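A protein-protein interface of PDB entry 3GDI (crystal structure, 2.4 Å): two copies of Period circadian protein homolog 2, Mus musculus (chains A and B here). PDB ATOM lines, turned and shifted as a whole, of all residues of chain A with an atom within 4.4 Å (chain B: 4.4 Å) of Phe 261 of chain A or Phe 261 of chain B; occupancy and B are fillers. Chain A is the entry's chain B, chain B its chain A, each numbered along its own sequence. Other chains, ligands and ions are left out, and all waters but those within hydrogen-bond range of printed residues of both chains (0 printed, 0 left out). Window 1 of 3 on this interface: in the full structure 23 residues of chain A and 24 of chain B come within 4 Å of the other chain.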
ATOM      1  N   THR A 170      19.410   9.943  26.322  1.00  0.00           N
ATOM      2  CA  THR A 170      19.656   9.819  24.902  1.00  0.00           C
ATOM      3  C   THR A 170      18.686  10.756  24.193  1.00  0.00           C
ATOM      4  O   THR A 170      17.542  10.917  24.631  1.00  0.00           O
ATOM      5  CB  THR A 170      19.388   8.382  24.433  1.00  0.00           C
ATOM      6  OG1 THR A 170      19.961   7.466  25.362  1.00  0.00           O
ATOM      7  CG2 THR A 170      19.998   8.135  23.091  1.00  0.00           C
ATOM      8  N   HIS A 171      19.149  11.409  23.131  1.00  0.00           N
ATOM      9  CA  HIS A 171      18.271  12.279  22.357  1.00  0.00           C
ATOM     10  C   HIS A 171      18.674  12.261  20.892  1.00  0.00           C
ATOM     11  O   HIS A 171      19.806  11.961  20.553  1.00  0.00           O
ATOM     12  CB  HIS A 171      18.199  13.718  22.919  1.00  0.00           C
ATOM     13  CG  HIS A 171      19.499  14.471  22.917  1.00  0.00           C
ATOM     14  ND1 HIS A 171      20.380  14.445  23.979  1.00  0.00           N
ATOM     15  CD2 HIS A 171      20.024  15.334  22.016  1.00  0.00           C
ATOM     16  CE1 HIS A 171      21.386  15.263  23.734  1.00  0.00           C
ATOM     17  NE2 HIS A 171      21.196  15.816  22.550  1.00  0.00           N
ATOM     18  N   THR A 172      17.715  12.539  20.027  1.00  0.00           N
ATOM     19  CA  THR A 172      17.942  12.531  18.599  1.00  0.00           C
ATOM     20  C   THR A 172      18.491  13.873  18.126  1.00  0.00           C
ATOM     21  O   THR A 172      18.485  14.845  18.877  1.00  0.00           O
ATOM     22  CB  THR A 172      16.628  12.161  17.885  1.00  0.00           C
ATOM     23  OG1 THR A 172      15.522  12.804  18.536  1.00  0.00           O
ATOM     24  CG2 THR A 172      16.405  10.651  17.959  1.00  0.00           C
ATOM     25  N   GLN A 178      14.828  10.747  23.439  1.00  0.00           N
ATOM     26  CA  GLN A 178      14.265   9.540  22.834  1.00  0.00           C
ATOM     27  C   GLN A 178      14.186   8.524  23.970  1.00  0.00           C
ATOM     28  O   GLN A 178      13.414   7.569  23.925  1.00  0.00           O
ATOM     29  CB  GLN A 178      15.157   8.973  21.725  1.00  0.00           C
ATOM     30  CG  GLN A 178      16.355   8.208  22.251  1.00  0.00           C
ATOM     31  CD  GLN A 178      16.124   6.701  22.370  1.00  0.00           C
ATOM     32  OE1 GLN A 178      16.872   6.002  23.070  1.00  0.00           O
ATOM     33  NE2 GLN A 178      15.126   6.190  21.663  1.00  0.00           N
ATOM     34  N   SER A 250      28.287  10.052  21.162  1.00  0.00           N
ATOM     35  CA  SER A 250      27.292   9.947  20.108  1.00  0.00           C
ATOM     36  C   SER A 250      27.328   8.622  19.362  1.00  0.00           C
ATOM     37  O   SER A 250      28.337   7.910  19.373  1.00  0.00           O
ATOM     38  CB  SER A 250      27.446  11.095  19.104  1.00  0.00           C
ATOM     39  OG  SER A 250      28.642  10.986  18.353  1.00  0.00           O
ATOM     40  N   PHE A 251      26.196   8.289  18.750  1.00  0.00           N
ATOM     41  CA  PHE A 251      26.065   7.085  17.951  1.00  0.00           C
ATOM     42  C   PHE A 251      25.998   7.582  16.504  1.00  0.00           C
ATOM     43  O   PHE A 251      25.058   8.284  16.107  1.00  0.00           O
ATOM     44  CB  PHE A 251      24.793   6.317  18.315  1.00  0.00           C
ATOM     45  CG  PHE A 251      24.866   5.600  19.647  1.00  0.00           C
ATOM     46  CD1 PHE A 251      26.065   5.071  20.106  1.00  0.00           C
ATOM     47  CD2 PHE A 251      23.719   5.400  20.407  1.00  0.00           C
ATOM     48  CE1 PHE A 251      26.116   4.351  21.305  1.00  0.00           C
ATOM     49  CE2 PHE A 251      23.763   4.684  21.600  1.00  0.00           C
ATOM     50  CZ  PHE A 251      24.959   4.156  22.050  1.00  0.00           C
ATOM     51  N   ILE A 259      25.221  11.567  12.836  1.00  0.00           N
ATOM     52  CA  ILE A 259      24.863  11.180  14.195  1.00  0.00           C
ATOM     53  C   ILE A 259      23.373  10.855  14.280  1.00  0.00           C
ATOM     54  O   ILE A 259      22.529  11.632  13.824  1.00  0.00           O
ATOM     55  CB  ILE A 259      25.223  12.310  15.199  1.00  0.00           C
ATOM     56  CG1 ILE A 259      26.744  12.329  15.416  1.00  0.00           C
ATOM     57  CG2 ILE A 259      24.480  12.123  16.518  1.00  0.00           C
ATOM     58  CD1 ILE A 259      27.237  13.442  16.332  1.00  0.00           C
ATOM     59  N   SER A 260      23.066   9.691  14.851  1.00  0.00           N
ATOM     60  CA  SER A 260      21.696   9.232  15.018  1.00  0.00           C
ATOM     61  C   SER A 260      21.229   9.520  16.448  1.00  0.00           C
ATOM     62  O   SER A 260      20.069   9.862  16.671  1.00  0.00           O
ATOM     63  CB  SER A 260      21.614   7.734  14.753  1.00  0.00           C
ATOM     64  OG  SER A 260      22.197   7.392  13.511  1.00  0.00           O
ATOM     65  N   PHE A 261      22.128   9.361  17.417  1.00  0.00           N
ATOM     66  CA  PHE A 261      21.787   9.634  18.815  1.00  0.00           C
ATOM     67  C   PHE A 261      22.943  10.250  19.590  1.00  0.00           C
ATOM     68  O   PHE A 261      24.106   9.882  19.394  1.00  0.00           O
ATOM     69  CB  PHE A 261      21.404   8.363  19.576  1.00  0.00           C
ATOM     70  CG  PHE A 261      20.345   7.534  18.915  1.00  0.00           C
ATOM     71  CD1 PHE A 261      20.694   6.510  18.035  1.00  0.00           C
ATOM     72  CD2 PHE A 261      18.999   7.750  19.197  1.00  0.00           C
ATOM     73  CE1 PHE A 261      19.714   5.710  17.449  1.00  0.00           C
ATOM     74  CE2 PHE A 261      18.013   6.960  18.620  1.00  0.00           C
ATOM     75  CZ  PHE A 261      18.370   5.934  17.742  1.00  0.00           C
ATOM     76  N   ILE A 262      22.611  11.186  20.471  1.00  0.00           N
ATOM     77  CA  ILE A 262      23.588  11.806  21.348  1.00  0.00           C
ATOM     78  C   ILE A 262      23.307  11.160  22.705  1.00  0.00           C
ATOM     79  O   ILE A 262      22.166  11.174  23.182  1.00  0.00           O
ATOM     80  CB  ILE A 262      23.370  13.326  21.491  1.00  0.00           C
ATOM     81  CG1 ILE A 262      23.689  14.046  20.177  1.00  0.00           C
ATOM     82  CG2 ILE A 262      24.231  13.864  22.625  1.00  0.00           C
ATOM     83  CD1 ILE A 262      22.609  13.914  19.140  1.00  0.00           C
ATOM     84  N   ILE A 263      24.329  10.587  23.326  1.00  0.00           N
ATOM     85  CA  ILE A 263      24.159   9.951  24.634  1.00  0.00           C
ATOM     86  C   ILE A 263      24.957  10.661  25.722  1.00  0.00           C
ATOM     87  O   ILE A 263      26.117  11.028  25.524  1.00  0.00           O
ATOM     88  CB  ILE A 263      24.585   8.494  24.581  1.00  0.00           C
ATOM     89  CG1 ILE A 263      25.934   8.376  23.870  1.00  0.00           C
ATOM     90  CG2 ILE A 263      23.538   7.690  23.864  1.00  0.00           C
ATOM     91  CD1 ILE A 263      26.353   6.951  23.590  1.00  0.00           C
ATOM     92  N   THR B 170      16.033   0.261  12.798  1.00  0.00           N
ATOM     93  CA  THR B 170      16.747   0.293  14.065  1.00  0.00           C
ATOM     94  C   THR B 170      15.900  -0.437  15.097  1.00  0.00           C
ATOM     95  O   THR B 170      14.688  -0.307  15.096  1.00  0.00           O
ATOM     96  CB  THR B 170      16.952   1.739  14.546  1.00  0.00           C
ATOM     97  OG1 THR B 170      17.688   2.465  13.558  1.00  0.00           O
ATOM     98  CG2 THR B 170      17.724   1.771  15.867  1.00  0.00           C
ATOM     99  N   HIS B 171      16.518  -1.234  15.950  1.00  0.00           N
ATOM    100  CA  HIS B 171      15.757  -1.898  16.989  1.00  0.00           C
ATOM    101  C   HIS B 171      16.524  -2.038  18.302  1.00  0.00           C
ATOM    102  O   HIS B 171      17.754  -2.049  18.327  1.00  0.00           O
ATOM    103  CB  HIS B 171      15.174  -3.250  16.517  1.00  0.00           C
ATOM    104  CG  HIS B 171      16.177  -4.310  16.164  1.00  0.00           C
ATOM    105  ND1 HIS B 171      16.624  -4.515  14.874  1.00  0.00           N
ATOM    106  CD2 HIS B 171      16.696  -5.319  16.902  1.00  0.00           C
ATOM    107  CE1 HIS B 171      17.364  -5.606  14.829  1.00  0.00           C
ATOM    108  NE2 HIS B 171      17.423  -6.116  16.047  1.00  0.00           N
ATOM    109  N   THR B 172      15.782  -2.076  19.400  1.00  0.00           N
ATOM    110  CA  THR B 172      16.370  -2.206  20.719  1.00  0.00           C
ATOM    111  C   THR B 172      16.702  -3.669  20.990  1.00  0.00           C
ATOM    112  O   THR B 172      16.303  -4.561  20.240  1.00  0.00           O
ATOM    113  CB  THR B 172      15.410  -1.653  21.813  1.00  0.00           C
ATOM    114  OG1 THR B 172      14.053  -1.943  21.456  1.00  0.00           O
ATOM    115  CG2 THR B 172      15.574  -0.154  21.967  1.00  0.00           C
ATOM    116  N   GLN B 178      12.593   0.456  16.638  1.00  0.00           N
ATOM    117  CA  GLN B 178      12.703   1.729  17.340  1.00  0.00           C
ATOM    118  C   GLN B 178      12.404   2.844  16.333  1.00  0.00           C
ATOM    119  O   GLN B 178      11.894   3.920  16.678  1.00  0.00           O
ATOM    120  CB  GLN B 178      14.114   1.912  17.928  1.00  0.00           C
ATOM    121  CG  GLN B 178      14.313   3.245  18.655  1.00  0.00           C
ATOM    122  CD  GLN B 178      14.764   4.361  17.709  1.00  0.00           C
ATOM    123  OE1 GLN B 178      14.628   5.557  18.011  1.00  0.00           O
ATOM    124  NE2 GLN B 178      15.325   3.974  16.575  1.00  0.00           N
ATOM    125  N   SER B 250      25.738  -2.217  15.142  1.00  0.00           N
ATOM    126  CA  SER B 250      25.149  -1.915  16.439  1.00  0.00           C
ATOM    127  C   SER B 250      25.728  -0.657  17.043  1.00  0.00           C
ATOM    128  O   SER B 250      26.830  -0.244  16.694  1.00  0.00           O
ATOM    129  CB  SER B 250      25.389  -3.071  17.413  1.00  0.00           C
ATOM    130  OG  SER B 250      26.768  -3.367  17.499  1.00  0.00           O
ATOM    131  N   PHE B 251      24.964  -0.035  17.933  1.00  0.00           N
ATOM    132  CA  PHE B 251      25.443   1.136  18.638  1.00  0.00           C
ATOM    133  C   PHE B 251      25.742   0.614  20.041  1.00  0.00           C
ATOM    134  O   PHE B 251      24.861   0.070  20.702  1.00  0.00           O
ATOM    135  CB  PHE B 251      24.382   2.239  18.676  1.00  0.00           C
ATOM    136  CG  PHE B 251      24.141   2.902  17.338  1.00  0.00           C
ATOM    137  CD1 PHE B 251      25.202   3.147  16.464  1.00  0.00           C
ATOM    138  CD2 PHE B 251      22.864   3.309  16.965  1.00  0.00           C
ATOM    139  CE1 PHE B 251      24.994   3.796  15.236  1.00  0.00           C
ATOM    140  CE2 PHE B 251      22.642   3.955  15.747  1.00  0.00           C
ATOM    141  CZ  PHE B 251      23.711   4.201  14.879  1.00  0.00           C
ATOM    142  N   ILE B 259      25.107  -3.200  24.195  1.00  0.00           N
ATOM    143  CA  ILE B 259      24.485  -2.770  22.954  1.00  0.00           C
ATOM    144  C   ILE B 259      23.172  -2.060  23.280  1.00  0.00           C
ATOM    145  O   ILE B 259      22.359  -2.595  24.040  1.00  0.00           O
ATOM    146  CB  ILE B 259      24.209  -3.997  22.030  1.00  0.00           C
ATOM    147  CG1 ILE B 259      25.498  -4.385  21.305  1.00  0.00           C
ATOM    148  CG2 ILE B 259      23.059  -3.702  21.061  1.00  0.00           C
ATOM    149  CD1 ILE B 259      25.315  -5.404  20.187  1.00  0.00           C
ATOM    150  N   SER B 260      22.984  -0.858  22.718  1.00  0.00           N
ATOM    151  CA  SER B 260      21.768  -0.069  22.921  1.00  0.00           C
ATOM    152  C   SER B 260      20.794  -0.185  21.738  1.00  0.00           C
ATOM    153  O   SER B 260      19.577  -0.153  21.933  1.00  0.00           O
ATOM    154  CB  SER B 260      22.105   1.404  23.126  1.00  0.00           C
ATOM    155  OG  SER B 260      22.926   1.599  24.256  1.00  0.00           O
ATOM    156  N   PHE B 261      21.328  -0.298  20.521  1.00  0.00           N
ATOM    157  CA  PHE B 261      20.508  -0.433  19.317  1.00  0.00           C
ATOM    158  C   PHE B 261      21.182  -1.348  18.297  1.00  0.00           C
ATOM    159  O   PHE B 261      22.397  -1.487  18.283  1.00  0.00           O
ATOM    160  CB  PHE B 261      20.314   0.906  18.594  1.00  0.00           C
ATOM    161  CG  PHE B 261      19.721   1.985  19.429  1.00  0.00           C
ATOM    162  CD1 PHE B 261      20.538   2.899  20.082  1.00  0.00           C
ATOM    163  CD2 PHE B 261      18.337   2.117  19.529  1.00  0.00           C
ATOM    164  CE1 PHE B 261      19.993   3.934  20.821  1.00  0.00           C
ATOM    165  CE2 PHE B 261      17.771   3.155  20.269  1.00  0.00           C
ATOM    166  CZ  PHE B 261      18.596   4.066  20.918  1.00  0.00           C
ATOM    167  N   ILE B 262      20.378  -1.945  17.426  1.00  0.00           N
ATOM    168  CA  ILE B 262      20.882  -2.789  16.349  1.00  0.00           C
ATOM    169  C   ILE B 262      20.398  -2.038  15.122  1.00  0.00           C
ATOM    170  O   ILE B 262      19.208  -1.752  15.032  1.00  0.00           O
ATOM    171  CB  ILE B 262      20.204  -4.164  16.323  1.00  0.00           C
ATOM    172  CG1 ILE B 262      20.430  -4.903  17.650  1.00  0.00           C
ATOM    173  CG2 ILE B 262      20.730  -4.965  15.137  1.00  0.00           C
ATOM    174  CD1 ILE B 262      21.820  -5.498  17.788  1.00  0.00           C
ATOM    175  N   ILE B 263      21.293  -1.695  14.197  1.00  0.00           N
ATOM    176  CA  ILE B 263      20.892  -0.981  12.986  1.00  0.00           C
ATOM    177  C   ILE B 263      21.155  -1.789  11.739  1.00  0.00           C
ATOM    178  O   ILE B 263      22.215  -2.394  11.598  1.00  0.00           O
ATOM    179  CB  ILE B 263      21.629   0.338  12.822  1.00  0.00           C
ATOM    180  CG1 ILE B 263      23.112   0.134  13.117  1.00  0.00           C
ATOM    181  CG2 ILE B 263      21.013   1.377  13.710  1.00  0.00           C
ATOM    182  CD1 ILE B 263      23.933   1.410  13.060  1.00  0.00           C
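The backbone NH (N) of Gln 178 of chain B is in hydrogen-bond range of the backbone carbonyl oxygen (O) of Thr 170 of chain B. The backbone carbonyl oxygen of Phe 251 of chain B lies within hydrogen-bond range of the backbone NH of Ser 260 of chain B, 2.9 Å away. O of Phe 261 of chain B sits at hydrogen-bond distance from N of Phe 251 of chain B. O of Thr 170 of chain A lies within hydrogen-bond range of N of Gln 178 of chain A (3.0 Å). O of Phe 251 of chain A is in hydrogen-bond range of N of Ser 260 of chain A, at 2.7 Å. The backbone carbonyl oxygen (O) of Phe 261 of chain A sits at hydrogen-bond distance from the backbone NH (N) of Phe 251 of chain A (2.7 Å).
Among the printed residues, pairs that only touch across the chains: Gln 178 of chain A with Gln 178 of chain B, Gln 178 of chain A with Phe 261 of chain B, Phe 251 of chain A with Phe 251 of chain B, Phe 251 of chain A with Ser 260 of chain B, Phe 251 of chain A with Phe 261 of chain B, Ser 260 of chain A with Phe 251 of chain B, Phe 261 of chain A with Gln 178 of chain B, Phe 261 of chain A with Phe 251 of chain B and Phe 261 of chain A with Phe 261 of chain B.
Printed residues of chain B within 4 Å of Phe 251 of chain A: Phe 251, Ser 260 and Phe 261. Of the printed residues of chain B, Ser 260 of chain A touches Phe 251. Ile 263 of chain A touches none of the printed residues of chain B. Of the printed residues of chain A, Ser 260 of chain B touches Phe 251. Phe 261 of chain B touches just these residues of chain A: Gln 178 (3.4 Å), Phe 251 (3.9 Å) and Phe 261 (3.7 Å). The nearest printed residue of chain A that does not touch Phe 261 of chain B is Thr 170 of chain A (4.8 Å). The nearest printed residue of chain A that does not touch Gln 178 of chain B is Thr 172 of chain A (5.4 Å).
Of the 11 printed residues of chain B, 4 touch a printed residue of chain A. Along chain B the printed residues that touch a printed residue of chain A span positions 178 to 261. Of the 11 printed residues of chain A, 4 touch a printed residue of chain B. Hydrophobic or aromatic side chains of chain A within 4 Å of the printed part of chain B: Phe 251 and Phe 261. Among the printed residues, 9 pairs touch across the chains. Among the printed residues, no Asp or Glu carboxylate lies within 4 Å of a Lys or Arg side-chain nitrogen of the other chain.
Gln 178 of chain B touches its own counterpart, Gln 178 of chain A. Phe 251 of chain A touches its own counterpart, Phe 251 of chain B. Phe 251 of chain A touches Ser 260 of chain B, and with the chains exchanged Ser 260 of chain A touches Phe 251 of chain B. Phe 251 of chain A touches Phe 261 of chain B, and with the chains exchanged Phe 261 of chain A touches Phe 251 of chain B. Positions printed for both chains: 170, 171, 172, 178, 250, 251, 259, 260, 261, 262 and 263.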
